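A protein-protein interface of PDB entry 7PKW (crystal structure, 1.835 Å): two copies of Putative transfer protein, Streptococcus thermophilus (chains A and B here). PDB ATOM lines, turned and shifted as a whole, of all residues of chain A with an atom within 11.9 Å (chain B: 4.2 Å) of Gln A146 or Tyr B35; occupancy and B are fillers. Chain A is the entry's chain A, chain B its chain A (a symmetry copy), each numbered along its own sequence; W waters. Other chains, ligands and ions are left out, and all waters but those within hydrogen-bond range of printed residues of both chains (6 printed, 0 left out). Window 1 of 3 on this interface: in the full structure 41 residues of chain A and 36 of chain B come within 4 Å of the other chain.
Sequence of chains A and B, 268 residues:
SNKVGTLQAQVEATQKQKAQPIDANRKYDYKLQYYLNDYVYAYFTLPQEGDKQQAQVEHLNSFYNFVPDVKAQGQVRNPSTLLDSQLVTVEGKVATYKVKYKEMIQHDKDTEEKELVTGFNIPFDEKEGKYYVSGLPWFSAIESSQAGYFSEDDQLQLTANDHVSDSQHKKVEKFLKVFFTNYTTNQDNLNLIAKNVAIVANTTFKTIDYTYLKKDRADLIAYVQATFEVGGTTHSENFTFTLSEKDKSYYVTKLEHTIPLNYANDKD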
ATOM      1  N   ASP A  84       1.145   2.464 -22.650  1.00  0.00           N
ATOM      2  CA  ASP A  84       1.945   3.181 -21.620  1.00  0.00           C
ATOM      3  C   ASP A  84       1.175   4.407 -21.128  1.00  0.00           C
ATOM      4  O   ASP A  84       0.354   4.976 -21.862  1.00  0.00           O
ATOM      5  CB  ASP A  84       3.302   3.634 -22.174  1.00  0.00           C
ATOM      6  CG  ASP A  84       4.333   3.975 -21.112  1.00  0.00           C
ATOM      7  OD1 ASP A  84       4.189   3.539 -19.969  1.00  0.00           O
ATOM      8  OD2 ASP A  84       5.277   4.664 -21.463  1.00  0.00           O
ATOM      9  N   SER A  85       1.444   4.811 -19.911  1.00  0.00           N
ATOM     10  CA  SER A  85       0.828   6.017 -19.328  1.00  0.00           C
ATOM     11  C   SER A  85       1.775   6.596 -18.282  1.00  0.00           C
ATOM     12  O   SER A  85       2.569   5.841 -17.657  1.00  0.00           O
ATOM     13  CB  SER A  85      -0.520   5.694 -18.768  1.00  0.00           C
ATOM     14  OG  SER A  85      -0.412   4.907 -17.593  1.00  0.00           O
ATOM     15  N   GLN A  86       1.768   7.905 -18.175  1.00  0.00           N
ATOM     16  CA  GLN A  86       2.592   8.657 -17.214  1.00  0.00           C
ATOM     17  C   GLN A  86       1.654   9.656 -16.556  1.00  0.00           C
ATOM     18  O   GLN A  86       1.098  10.521 -17.273  1.00  0.00           O
ATOM     19  CB  GLN A  86       3.771   9.336 -17.914  1.00  0.00           C
ATOM     20  CG  GLN A  86       4.706   8.398 -18.688  1.00  0.00           C
ATOM     21  CD  GLN A  86       5.856   9.183 -19.280  1.00  0.00           C
ATOM     22  OE1 GLN A  86       5.759  10.385 -19.481  1.00  0.00           O
ATOM     23  NE2 GLN A  86       7.012   8.555 -19.427  1.00  0.00           N
ATOM     24  N   LEU A  87       1.523   9.571 -15.232  1.00  0.00           N
ATOM     25  CA  LEU A  87       0.780  10.603 -14.454  1.00  0.00           C
ATOM     26  C   LEU A  87       1.687  11.807 -14.216  1.00  0.00           C
ATOM     27  O   LEU A  87       2.531  11.735 -13.321  1.00  0.00           O
ATOM     28  CB  LEU A  87       0.353   9.986 -13.133  1.00  0.00           C
ATOM     29  CG  LEU A  87      -0.280  10.976 -12.162  1.00  0.00           C
ATOM     30  CD1 LEU A  87      -1.453  11.672 -12.807  1.00  0.00           C
ATOM     31  CD2 LEU A  87      -0.732  10.265 -10.912  1.00  0.00           C
ATOM     32  N   VAL A  88       1.594  12.847 -15.028  1.00  0.00           N
ATOM     33  CA  VAL A  88       2.625  13.910 -14.957  1.00  0.00           C
ATOM     34  C   VAL A  88       2.219  14.963 -13.925  1.00  0.00           C
ATOM     35  O   VAL A  88       3.119  15.551 -13.332  1.00  0.00           O
ATOM     36  CB  VAL A  88       2.954  14.506 -16.332  1.00  0.00           C
ATOM     37  CG1 VAL A  88       3.712  13.492 -17.146  1.00  0.00           C
ATOM     38  CG2 VAL A  88       1.757  14.978 -17.134  1.00  0.00           C
ATOM     39  N   THR A  89       0.944  15.324 -13.816  1.00  0.00           N
ATOM     40  CA  THR A  89       0.531  16.386 -12.852  1.00  0.00           C
ATOM     41  C   THR A  89      -0.809  16.046 -12.226  1.00  0.00           C
ATOM     42  O   THR A  89      -1.650  15.371 -12.878  1.00  0.00           O
ATOM     43  CB  THR A  89       0.501  17.791 -13.477  1.00  0.00           C
ATOM     44  OG1 THR A  89      -0.506  17.800 -14.479  1.00  0.00           O
ATOM     45  CG2 THR A  89       1.834  18.188 -14.090  1.00  0.00           C
ATOM     46  N   THR A  96      -3.443  14.851 -15.047  1.00  0.00           N
ATOM     47  CA  THR A  96      -2.996  14.906 -16.443  1.00  0.00           C
ATOM     48  C   THR A  96      -2.027  13.766 -16.690  1.00  0.00           C
ATOM     49  O   THR A  96      -1.021  13.681 -15.967  1.00  0.00           O
ATOM     50  CB  THR A  96      -2.401  16.287 -16.748  1.00  0.00           C
ATOM     51  OG1 THR A  96      -3.421  17.273 -16.538  1.00  0.00           O
ATOM     52  CG2 THR A  96      -1.903  16.356 -18.172  1.00  0.00           C
ATOM     53  N   TYR A  97      -2.267  13.026 -17.759  1.00  0.00           N
ATOM     54  CA  TYR A  97      -1.460  11.882 -18.228  1.00  0.00           C
ATOM     55  C   TYR A  97      -0.909  12.178 -19.617  1.00  0.00           C
ATOM     56  O   TYR A  97      -1.609  12.833 -20.447  1.00  0.00           O
ATOM     57  CB  TYR A  97      -2.320  10.620 -18.309  1.00  0.00           C
ATOM     58  CG  TYR A  97      -2.522   9.929 -16.992  1.00  0.00           C
ATOM     59  CD1 TYR A  97      -3.488  10.334 -16.086  1.00  0.00           C
ATOM     60  CD2 TYR A  97      -1.729   8.849 -16.658  1.00  0.00           C
ATOM     61  CE1 TYR A  97      -3.664   9.674 -14.881  1.00  0.00           C
ATOM     62  CE2 TYR A  97      -1.866   8.211 -15.439  1.00  0.00           C
ATOM     63  CZ  TYR A  97      -2.839   8.627 -14.536  1.00  0.00           C
ATOM     64  OH  TYR A  97      -2.942   8.023 -13.312  1.00  0.00           O
ATOM     65  N   LYS A  98       0.242  11.561 -19.902  1.00  0.00           N
ATOM     66  CA  LYS A  98       0.703  11.202 -21.259  1.00  0.00           C
ATOM     67  C   LYS A  98       0.264   9.763 -21.496  1.00  0.00           C
ATOM     68  O   LYS A  98       0.557   8.890 -20.627  1.00  0.00           O
ATOM     69  CB  LYS A  98       2.221  11.375 -21.395  1.00  0.00           C
ATOM     70  CG  LYS A  98       2.700  12.808 -21.214  1.00  0.00           C
ATOM     71  CD  LYS A  98       4.182  12.948 -21.495  1.00  0.00           C
ATOM     72  CE  LYS A  98       4.676  14.323 -21.129  1.00  0.00           C
ATOM     73  NZ  LYS A  98       6.139  14.462 -21.317  1.00  0.00           N
ATOM     74  N   ILE A 142       0.354  16.400 -26.062  1.00  0.00           N
ATOM     75  CA  ILE A 142       1.491  16.093 -25.151  1.00  0.00           C
ATOM     76  C   ILE A 142       2.419  17.296 -25.169  1.00  0.00           C
ATOM     77  O   ILE A 142       2.722  17.756 -26.259  1.00  0.00           O
ATOM     78  CB  ILE A 142       2.170  14.776 -25.586  1.00  0.00           C
ATOM     79  CG1 ILE A 142       1.296  13.621 -25.086  1.00  0.00           C
ATOM     80  CG2 ILE A 142       3.608  14.690 -25.079  1.00  0.00           C
ATOM     81  CD1 ILE A 142       1.584  12.289 -25.694  1.00  0.00           C
ATOM     82  N   GLU A 143       2.803  17.791 -23.982  1.00  0.00           N
ATOM     83  CA  GLU A 143       3.795  18.879 -23.807  1.00  0.00           C
ATOM     84  C   GLU A 143       5.130  18.229 -23.399  1.00  0.00           C
ATOM     85  O   GLU A 143       5.135  17.361 -22.469  1.00  0.00           O
ATOM     86  CB  GLU A 143       3.330  19.853 -22.725  1.00  0.00           C
ATOM     87  CG  GLU A 143       2.215  20.783 -23.158  1.00  0.00           C
ATOM     88  CD  GLU A 143       1.978  21.893 -22.143  1.00  0.00           C
ATOM     89  OE1 GLU A 143       1.758  21.572 -20.971  1.00  0.00           O
ATOM     90  OE2 GLU A 143       2.050  23.082 -22.517  1.00  0.00           O
ATOM     91  N   SER A 144       6.206  18.563 -24.082  1.00  0.00           N
ATOM     92  CA  SER A 144       7.568  18.066 -23.712  1.00  0.00           C
ATOM     93  C   SER A 144       8.088  18.928 -22.557  1.00  0.00           C
ATOM     94  O   SER A 144       7.913  20.147 -22.619  1.00  0.00           O
ATOM     95  CB  SER A 144       8.512  18.108 -24.882  1.00  0.00           C
ATOM     96  OG  SER A 144       9.814  17.759 -24.443  1.00  0.00           O
ATOM     97  N   SER A 145       8.781  18.364 -21.578  1.00  0.00           N
ATOM     98  CA  SER A 145       9.471  19.164 -20.524  1.00  0.00           C
ATOM     99  C   SER A 145      10.936  19.442 -20.933  1.00  0.00           C
ATOM    100  O   SER A 145      11.695  19.907 -20.038  1.00  0.00           O
ATOM    101  CB  SER A 145       9.417  18.497 -19.172  1.00  0.00           C
ATOM    102  OG  SER A 145       8.097  18.559 -18.609  1.00  0.00           O
ATOM    103  N   GLN A 146      11.298  19.203 -22.206  1.00  0.00           N
ATOM    104  CA  GLN A 146      12.691  19.437 -22.700  1.00  0.00           C
ATOM    105  C   GLN A 146      13.003  20.929 -22.727  1.00  0.00           C
ATOM    106  O   GLN A 146      12.284  21.703 -23.395  1.00  0.00           O
ATOM    107  CB  GLN A 146      12.933  18.840 -24.093  1.00  0.00           C
ATOM    108  CG  GLN A 146      14.365  19.084 -24.554  1.00  0.00           C
ATOM    109  CD  GLN A 146      15.399  18.470 -23.623  1.00  0.00           C
ATOM    110  OE1 GLN A 146      15.289  17.315 -23.252  1.00  0.00           O
ATOM    111  NE2 GLN A 146      16.505  19.159 -23.367  1.00  0.00           N
ATOM    112  N   ALA A 147      14.060  21.372 -22.050  1.00  0.00           N
ATOM    113  CA  ALA A 147      14.500  22.774 -22.148  1.00  0.00           C
ATOM    114  C   ALA A 147      15.238  22.975 -23.481  1.00  0.00           C
ATOM    115  O   ALA A 147      15.889  22.016 -23.983  1.00  0.00           O
ATOM    116  CB  ALA A 147      15.345  23.173 -20.975  1.00  0.00           C
ATOM    117  N   GLY A 148      15.224  24.215 -23.976  1.00  0.00           N
ATOM    118  CA  GLY A 148      16.068  24.661 -25.108  1.00  0.00           C
ATOM    119  C   GLY A 148      16.521  26.102 -24.962  1.00  0.00           C
ATOM    120  O   GLY A 148      16.471  26.673 -23.815  1.00  0.00           O
ATOM    121  N   TYR A 149      16.985  26.661 -26.078  1.00  0.00           N
ATOM    122  CA  TYR A 149      17.537  28.027 -26.187  1.00  0.00           C
ATOM    123  C   TYR A 149      18.649  28.206 -25.150  1.00  0.00           C
ATOM    124  O   TYR A 149      18.457  28.949 -24.170  1.00  0.00           O
ATOM    125  CB  TYR A 149      16.420  29.053 -25.967  1.00  0.00           C
ATOM    126  CG  TYR A 149      15.240  28.863 -26.884  1.00  0.00           C
ATOM    127  CD1 TYR A 149      15.407  28.857 -28.263  1.00  0.00           C
ATOM    128  CD2 TYR A 149      13.956  28.687 -26.387  1.00  0.00           C
ATOM    129  CE1 TYR A 149      14.334  28.681 -29.124  1.00  0.00           C
ATOM    130  CE2 TYR A 149      12.874  28.509 -27.237  1.00  0.00           C
ATOM    131  CZ  TYR A 149      13.061  28.511 -28.610  1.00  0.00           C
ATOM    132  OH  TYR A 149      12.006  28.342 -29.461  1.00  0.00           O
ATOM    133  N   PHE A 150      19.767  27.509 -25.307  1.00  0.00           N
ATOM    134  CA  PHE A 150      20.946  27.733 -24.441  1.00  0.00           C
ATOM    135  C   PHE A 150      21.964  28.653 -25.127  1.00  0.00           C
ATOM    136  O   PHE A 150      22.131  28.586 -26.346  1.00  0.00           O
ATOM    137  CB  PHE A 150      21.583  26.392 -24.103  1.00  0.00           C
ATOM    138  CG  PHE A 150      20.661  25.464 -23.354  1.00  0.00           C
ATOM    139  CD1 PHE A 150      20.493  25.584 -21.985  1.00  0.00           C
ATOM    140  CD2 PHE A 150      19.968  24.492 -24.044  1.00  0.00           C
ATOM    141  CE1 PHE A 150      19.660  24.707 -21.301  1.00  0.00           C
ATOM    142  CE2 PHE A 150      19.119  23.624 -23.368  1.00  0.00           C
ATOM    143  CZ  PHE A 150      18.963  23.758 -22.011  1.00  0.00           C
ATOM    144  N   LYS B  31       6.887  15.526 -13.477  1.00  0.00           N
ATOM    145  CA  LYS B  31       7.439  15.790 -14.819  1.00  0.00           C
ATOM    146  C   LYS B  31       8.926  15.423 -14.828  1.00  0.00           C
ATOM    147  O   LYS B  31       9.376  14.781 -15.807  1.00  0.00           O
ATOM    148  CB  LYS B  31       7.190  17.238 -15.240  1.00  0.00           C
ATOM    149  CG  LYS B  31       5.735  17.587 -15.538  1.00  0.00           C
ATOM    150  CD  LYS B  31       5.635  19.031 -15.973  1.00  0.00           C
ATOM    151  CE  LYS B  31       4.252  19.453 -16.355  1.00  0.00           C
ATOM    152  NZ  LYS B  31       4.275  20.901 -16.690  1.00  0.00           N
ATOM    153  N   LEU B  32       9.664  15.779 -13.780  1.00  0.00           N
ATOM    154  CA  LEU B  32      11.124  15.484 -13.683  1.00  0.00           C
ATOM    155  C   LEU B  32      11.319  13.970 -13.678  1.00  0.00           C
ATOM    156  O   LEU B  32      12.171  13.482 -14.409  1.00  0.00           O
ATOM    157  CB  LEU B  32      11.752  16.095 -12.434  1.00  0.00           C
ATOM    158  CG  LEU B  32      13.231  15.751 -12.216  1.00  0.00           C
ATOM    159  CD1 LEU B  32      14.067  16.093 -13.454  1.00  0.00           C
ATOM    160  CD2 LEU B  32      13.753  16.489 -11.002  1.00  0.00           C
ATOM    161  N   GLN B  33      10.609  13.239 -12.826  1.00  0.00           N
ATOM    162  CA  GLN B  33      10.798  11.771 -12.724  1.00  0.00           C
ATOM    163  C   GLN B  33      10.532  11.124 -14.082  1.00  0.00           C
ATOM    164  O   GLN B  33      11.359  10.274 -14.513  1.00  0.00           O
ATOM    165  CB  GLN B  33       9.943  11.154 -11.617  1.00  0.00           C
ATOM    166  CG  GLN B  33      10.295  11.675 -10.245  1.00  0.00           C
ATOM    167  CD  GLN B  33       9.515  12.881  -9.779  1.00  0.00           C
ATOM    168  OE1 GLN B  33       9.169  13.765 -10.574  1.00  0.00           O
ATOM    169  NE2 GLN B  33       9.265  12.944  -8.465  1.00  0.00           N
ATOM    170  N   TYR B  34       9.488  11.539 -14.797  1.00  0.00           N
ATOM    171  CA  TYR B  34       9.182  10.898 -16.096  1.00  0.00           C
ATOM    172  C   TYR B  34      10.150  11.395 -17.189  1.00  0.00           C
ATOM    173  O   TYR B  34      10.442  10.599 -18.079  1.00  0.00           O
ATOM    174  CB  TYR B  34       7.723  11.138 -16.476  1.00  0.00           C
ATOM    175  CG  TYR B  34       6.778  10.210 -15.738  1.00  0.00           C
ATOM    176  CD1 TYR B  34       6.779   8.831 -15.940  1.00  0.00           C
ATOM    177  CD2 TYR B  34       5.824  10.741 -14.873  1.00  0.00           C
ATOM    178  CE1 TYR B  34       5.885   8.001 -15.275  1.00  0.00           C
ATOM    179  CE2 TYR B  34       4.938   9.934 -14.209  1.00  0.00           C
ATOM    180  CZ  TYR B  34       4.941   8.576 -14.439  1.00  0.00           C
ATOM    181  OH  TYR B  34       3.980   7.849 -13.794  1.00  0.00           O
ATOM    182  N   TYR B  35      10.601  12.636 -17.137  1.00  0.00           N
ATOM    183  CA  TYR B  35      11.661  13.124 -18.046  1.00  0.00           C
ATOM    184  C   TYR B  35      12.900  12.212 -17.937  1.00  0.00           C
ATOM    185  O   TYR B  35      13.495  11.771 -18.944  1.00  0.00           O
ATOM    186  CB  TYR B  35      11.972  14.579 -17.730  1.00  0.00           C
ATOM    187  CG  TYR B  35      13.099  15.086 -18.570  1.00  0.00           C
ATOM    188  CD1 TYR B  35      12.869  15.537 -19.857  1.00  0.00           C
ATOM    189  CD2 TYR B  35      14.399  15.111 -18.080  1.00  0.00           C
ATOM    190  CE1 TYR B  35      13.922  16.002 -20.646  1.00  0.00           C
ATOM    191  CE2 TYR B  35      15.464  15.535 -18.876  1.00  0.00           C
ATOM    192  CZ  TYR B  35      15.223  16.000 -20.156  1.00  0.00           C
ATOM    193  OH  TYR B  35      16.265  16.413 -20.978  1.00  0.00           O
ATOM    194  N   LEU B  36      13.349  11.959 -16.704  1.00  0.00           N
ATOM    195  CA  LEU B  36      14.527  11.121 -16.462  1.00  0.00           C
ATOM    196  C   LEU B  36      14.271   9.688 -16.935  1.00  0.00           C
ATOM    197  O   LEU B  36      15.139   9.111 -17.581  1.00  0.00           O
ATOM    198  CB  LEU B  36      14.858  11.229 -14.990  1.00  0.00           C
ATOM    199  CG  LEU B  36      15.343  12.593 -14.516  1.00  0.00           C
ATOM    200  CD1 LEU B  36      15.313  12.665 -12.990  1.00  0.00           C
ATOM    201  CD2 LEU B  36      16.731  12.888 -15.037  1.00  0.00           C
ATOM    202  N   ASN B  37      13.076   9.135 -16.701  1.00  0.00           N
ATOM    203  CA  ASN B  37      12.705   7.793 -17.217  1.00  0.00           C
ATOM    204  C   ASN B  37      12.829   7.777 -18.748  1.00  0.00           C
ATOM    205  O   ASN B  37      13.390   6.788 -19.291  1.00  0.00           O
ATOM    206  CB  ASN B  37      11.277   7.402 -16.835  1.00  0.00           C
ATOM    207  CG  ASN B  37      11.116   6.948 -15.388  1.00  0.00           C
ATOM    208  OD1 ASN B  37      12.073   6.898 -14.572  1.00  0.00           O
ATOM    209  ND2 ASN B  37       9.869   6.614 -15.056  1.00  0.00           N
ATOM    210  N   ASP B  38      12.337   8.828 -19.411  1.00  0.00           N
ATOM    211  CA  ASP B  38      12.398   8.937 -20.895  1.00  0.00           C
ATOM    212  C   ASP B  38      13.866   9.021 -21.380  1.00  0.00           C
ATOM    213  O   ASP B  38      14.171   8.375 -22.390  1.00  0.00           O
ATOM    214  CB  ASP B  38      11.641  10.143 -21.442  1.00  0.00           C
ATOM    215  CG  ASP B  38      10.143  10.142 -21.187  1.00  0.00           C
ATOM    216  OD1 ASP B  38       9.626   9.098 -20.895  1.00  0.00           O
ATOM    217  OD2 ASP B  38       9.537  11.204 -21.305  1.00  0.00           O
ATOM    218  N   TYR B  39      14.738   9.696 -20.644  1.00  0.00           N
ATOM    219  CA  TYR B  39      16.186   9.753 -20.983  1.00  0.00           C
ATOM    220  C   TYR B  39      16.759   8.349 -20.849  1.00  0.00           C
ATOM    221  O   TYR B  39      17.449   7.892 -21.765  1.00  0.00           O
ATOM    222  CB  TYR B  39      16.967  10.720 -20.093  1.00  0.00           C
ATOM    223  CG  TYR B  39      18.451  10.688 -20.395  1.00  0.00           C
ATOM    224  CD1 TYR B  39      18.962  11.232 -21.566  1.00  0.00           C
ATOM    225  CD2 TYR B  39      19.342  10.133 -19.502  1.00  0.00           C
ATOM    226  CE1 TYR B  39      20.323  11.206 -21.836  1.00  0.00           C
ATOM    227  CE2 TYR B  39      20.713  10.102 -19.755  1.00  0.00           C
ATOM    228  CZ  TYR B  39      21.205  10.643 -20.924  1.00  0.00           C
ATOM    229  OH  TYR B  39      22.556  10.647 -21.157  1.00  0.00           O
ATOM    230  N   SER B  62      18.637  15.001 -28.265  1.00  0.00           N
ATOM    231  CA  SER B  62      17.692  16.108 -27.988  1.00  0.00           C
ATOM    232  C   SER B  62      17.604  16.361 -26.477  1.00  0.00           C
ATOM    233  O   SER B  62      17.080  17.444 -26.085  1.00  0.00           O
ATOM    234  CB  SER B  62      16.313  15.859 -28.603  1.00  0.00           C
ATOM    235  OG  SER B  62      15.528  14.905 -27.850  1.00  0.00           O
ATOM    236  N   PHE B  63      18.026  15.407 -25.635  1.00  0.00           N
ATOM    237  CA  PHE B  63      17.908  15.578 -24.156  1.00  0.00           C
ATOM    238  C   PHE B  63      18.953  16.555 -23.632  1.00  0.00           C
ATOM    239  O   PHE B  63      18.726  17.189 -22.560  1.00  0.00           O
ATOM    240  CB  PHE B  63      18.003  14.218 -23.456  1.00  0.00           C
ATOM    241  CG  PHE B  63      16.740  13.395 -23.538  1.00  0.00           C
ATOM    242  CD1 PHE B  63      16.466  12.622 -24.653  1.00  0.00           C
ATOM    243  CD2 PHE B  63      15.827  13.390 -22.480  1.00  0.00           C
ATOM    244  CE1 PHE B  63      15.320  11.838 -24.715  1.00  0.00           C
ATOM    245  CE2 PHE B  63      14.670  12.634 -22.564  1.00  0.00           C
ATOM    246  CZ  PHE B  63      14.413  11.849 -23.676  1.00  0.00           C
ATOM    247  N   LYS B 130      11.621  23.755 -17.205  1.00  0.00           N
ATOM    248  CA  LYS B 130      11.913  22.631 -18.130  1.00  0.00           C
ATOM    249  C   LYS B 130      13.250  21.973 -17.737  1.00  0.00           C
ATOM    250  O   LYS B 130      14.007  22.556 -17.068  1.00  0.00           O
ATOM    251  CB  LYS B 130      11.901  23.117 -19.583  1.00  0.00           C
ATOM    252  CG  LYS B 130      10.513  23.426 -20.153  1.00  0.00           C
ATOM    253  CD  LYS B 130      10.628  24.390 -21.311  1.00  0.00           C
ATOM    254  CE  LYS B 130       9.315  25.023 -21.736  1.00  0.00           C
ATOM    255  NZ  LYS B 130       8.320  23.984 -22.057  1.00  0.00           N
ATOM    256  N   TYR B 131      13.539  20.817 -18.279  1.00  0.00           N
ATOM    257  CA  TYR B 131      14.681  19.989 -17.822  1.00  0.00           C
ATOM    258  C   TYR B 131      15.616  19.721 -18.985  1.00  0.00           C
ATOM    259  O   TYR B 131      15.194  19.704 -20.133  1.00  0.00           O
ATOM    260  CB  TYR B 131      14.175  18.682 -17.222  1.00  0.00           C
ATOM    261  CG  TYR B 131      13.262  18.938 -16.056  1.00  0.00           C
ATOM    262  CD1 TYR B 131      13.740  19.571 -14.938  1.00  0.00           C
ATOM    263  CD2 TYR B 131      11.910  18.625 -16.104  1.00  0.00           C
ATOM    264  CE1 TYR B 131      12.922  19.846 -13.852  1.00  0.00           C
ATOM    265  CE2 TYR B 131      11.061  18.953 -15.049  1.00  0.00           C
ATOM    266  CZ  TYR B 131      11.573  19.560 -13.919  1.00  0.00           C
ATOM    267  OH  TYR B 131      10.813  19.829 -12.815  1.00  0.00           O
ATOM    268  N   TYR B 132      16.869  19.419 -18.649  1.00  0.00           N
ATOM    269  CA  TYR B 132      17.841  18.915 -19.644  1.00  0.00           C
ATOM    270  C   TYR B 132      18.913  18.087 -18.929  1.00  0.00           C
ATOM    271  O   TYR B 132      19.150  18.290 -17.740  1.00  0.00           O
ATOM    272  CB  TYR B 132      18.526  20.067 -20.368  1.00  0.00           C
ATOM    273  CG  TYR B 132      19.268  21.079 -19.522  1.00  0.00           C
ATOM    274  CD1 TYR B 132      18.615  22.110 -18.874  1.00  0.00           C
ATOM    275  CD2 TYR B 132      20.661  21.069 -19.437  1.00  0.00           C
ATOM    276  CE1 TYR B 132      19.311  23.087 -18.163  1.00  0.00           C
ATOM    277  CE2 TYR B 132      21.356  22.009 -18.684  1.00  0.00           C
ATOM    278  CZ  TYR B 132      20.685  23.042 -18.076  1.00  0.00           C
ATOM    279  OH  TYR B 132      21.339  23.982 -17.317  1.00  0.00           O
ATOM    280  N   VAL B 133      19.551  17.221 -19.688  1.00  0.00           N
ATOM    281  CA  VAL B 133      20.754  16.472 -19.245  1.00  0.00           C
ATOM    282  C   VAL B 133      21.955  17.338 -19.606  1.00  0.00           C
ATOM    283  O   VAL B 133      21.995  17.937 -20.756  1.00  0.00           O
ATOM    284  CB  VAL B 133      20.790  15.095 -19.915  1.00  0.00           C
ATOM    285  CG1 VAL B 133      22.035  14.325 -19.492  1.00  0.00           C
ATOM    286  CG2 VAL B 133      19.548  14.304 -19.624  1.00  0.00           C
HETATM  287  O   HOH W   1       9.830  21.852 -24.197  1.00  0.00           O
HETATM  288  O   HOH W   2       6.961  10.340 -22.715  1.00  0.00           O
HETATM  289  O   HOH W   3       7.488  12.431 -19.871  1.00  0.00           O
HETATM  290  O   HOH W   4       3.704   5.348 -14.568  1.00  0.00           O
HETATM  291  O   HOH W   5      14.146  15.583 -25.251  1.00  0.00           O
HETATM  292  O   HOH W   6       8.005   5.950 -17.506  1.00  0.00           O
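The backbone carbonyl oxygen (O) of Phe B63 lies within hydrogen-bond range of the side-chain amide nitrogen (NE2) of Gln A146 (3.1 Å). OH of Tyr B34 lies within hydrogen-bond range of N of Leu A87, at 3.3 Å. NE2 of Gln A86 lies within hydrogen-bond range of OD1 of Asp B38 (3.0 Å). O of Tyr B131 is in hydrogen-bond range of N of Ala A147, 2.8 Å away. O of Ser B62 sits close to NE2 of Gln A146 (3.3 Å). OE1 of Gln A146 lies within hydrogen-bond range of OH of Tyr B35 (2.6 Å). The backbone NH (N) of Tyr B131 is in hydrogen-bond range of the backbone carbonyl oxygen (O) of Ser A145.
The backbone carbonyl oxygen (O) of Lys A98 is in hydrogen-bond range of the backbone NH (N) of Gln A86. The side-chain hydroxyl (OH) of Tyr B35 sits at hydrogen-bond distance from the backbone carbonyl oxygen (O) of Phe B63, 3.0 Å away. O of Phe B63 lies within hydrogen-bond range of N of Val B133 (3.0 Å). O of Thr A96 lies within hydrogen-bond range of N of Val A88, 2.9 Å away. The backbone NH of Gln A146 sits at hydrogen-bond distance from the side-chain hydroxyl of Ser A144 (3.0 Å). The backbone carbonyl oxygen (O) of Thr A89 lies within hydrogen-bond range of the backbone NH (N) of Thr A96.
Among the printed residues, pairs that only touch across the chains: Ser A145 with Lys B130, Gln A86 with Tyr B34, Gln A146 with Tyr B131, Thr A89 with Lys B31, Phe A150 with Tyr B132, Ser A145 with Lys B31, Ala A147 with Lys B130, Gln A146 with Tyr B132, Val A88 with Lys B31, Gln A146 with Lys B130 and Ser A144 with Lys B130.
Gln A146 touches just these residues of chain B: Tyr B35 (2.6 Å), Ser B62 (3.2 Å), Phe B63 (3.1 Å), Lys B130 (3.8 Å), Tyr B131 (3.5 Å) and Tyr B132 (3.7 Å). No residue of chain A comes within 4 Å of Leu B32. No residue of chain A comes within 4 Å of Leu B36. No residue of chain A comes within 4 Å of Asn B37. Asp B38 touches one residue of chain A. No residue of chain A comes within 4 Å of Val B133. Printed residues of chain A within 4 Å of Tyr B132: Gln A146 (3.7 Å) and Phe A150 (3.5 Å). Of the printed residues of chain B, Thr A89 touches Lys B31. Of the printed residues of chain B, Ala A147 touches Lys B130 and Tyr B131. Ile A142 touches none of the printed residues of chain B. Glu A143 touches none of the printed residues of chain B. The nearest residue of chain A that does not touch Tyr B35 is Ser A145 (4.5 Å).
Of the 15 printed residues of chain B, 9 touch a printed residue of chain A. Printed residues of chain B that touch a printed residue of chain A: Lys B31, Tyr B34, Tyr B35, Asp B38, Ser B62, Phe B63, Lys B130, Tyr B131 and Tyr B132. Hydrophobic or aromatic side chains of chain B within 4 Å of the printed part of chain A: Tyr B34, Tyr B35, Tyr B131 and Tyr B132. Among the printed residues, 18 pairs touch across the chains. Among the printed residues, no Asp or Glu carboxylate lies within 4 Å of a Lys or Arg side-chain nitrogen of the other chain.
No position is printed for both chains.
Water W1 lies within hydrogen-bond range of O of Gln A146 (2.6 Å), O of Ser A144 (3.0 Å) and NZ of Lys B130 (3.4 Å). Water W4 lies within hydrogen-bond range of the side-chain hydroxyl (OH) of Tyr B34 and the backbone carbonyl oxygen (O) of Ser A85. Water W3 lies within hydrogen-bond range of OE1 of Gln A86, OD2 of Asp B38 and NZ of Lys A98. Water W5 lies within hydrogen-bond range of the side-chain amide oxygen (OE1) of Gln A146 (2.9 Å) and the side-chain hydroxyl (OG) of Ser B62 (3.0 Å). Water W2 bridges OD2 of Asp B38 and OE1 of Gln A86. Water W6 lies within hydrogen-bond range of ND2 of Asn B37 (3.1 Å) and NE2 of Gln A86 (3.4 Å).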
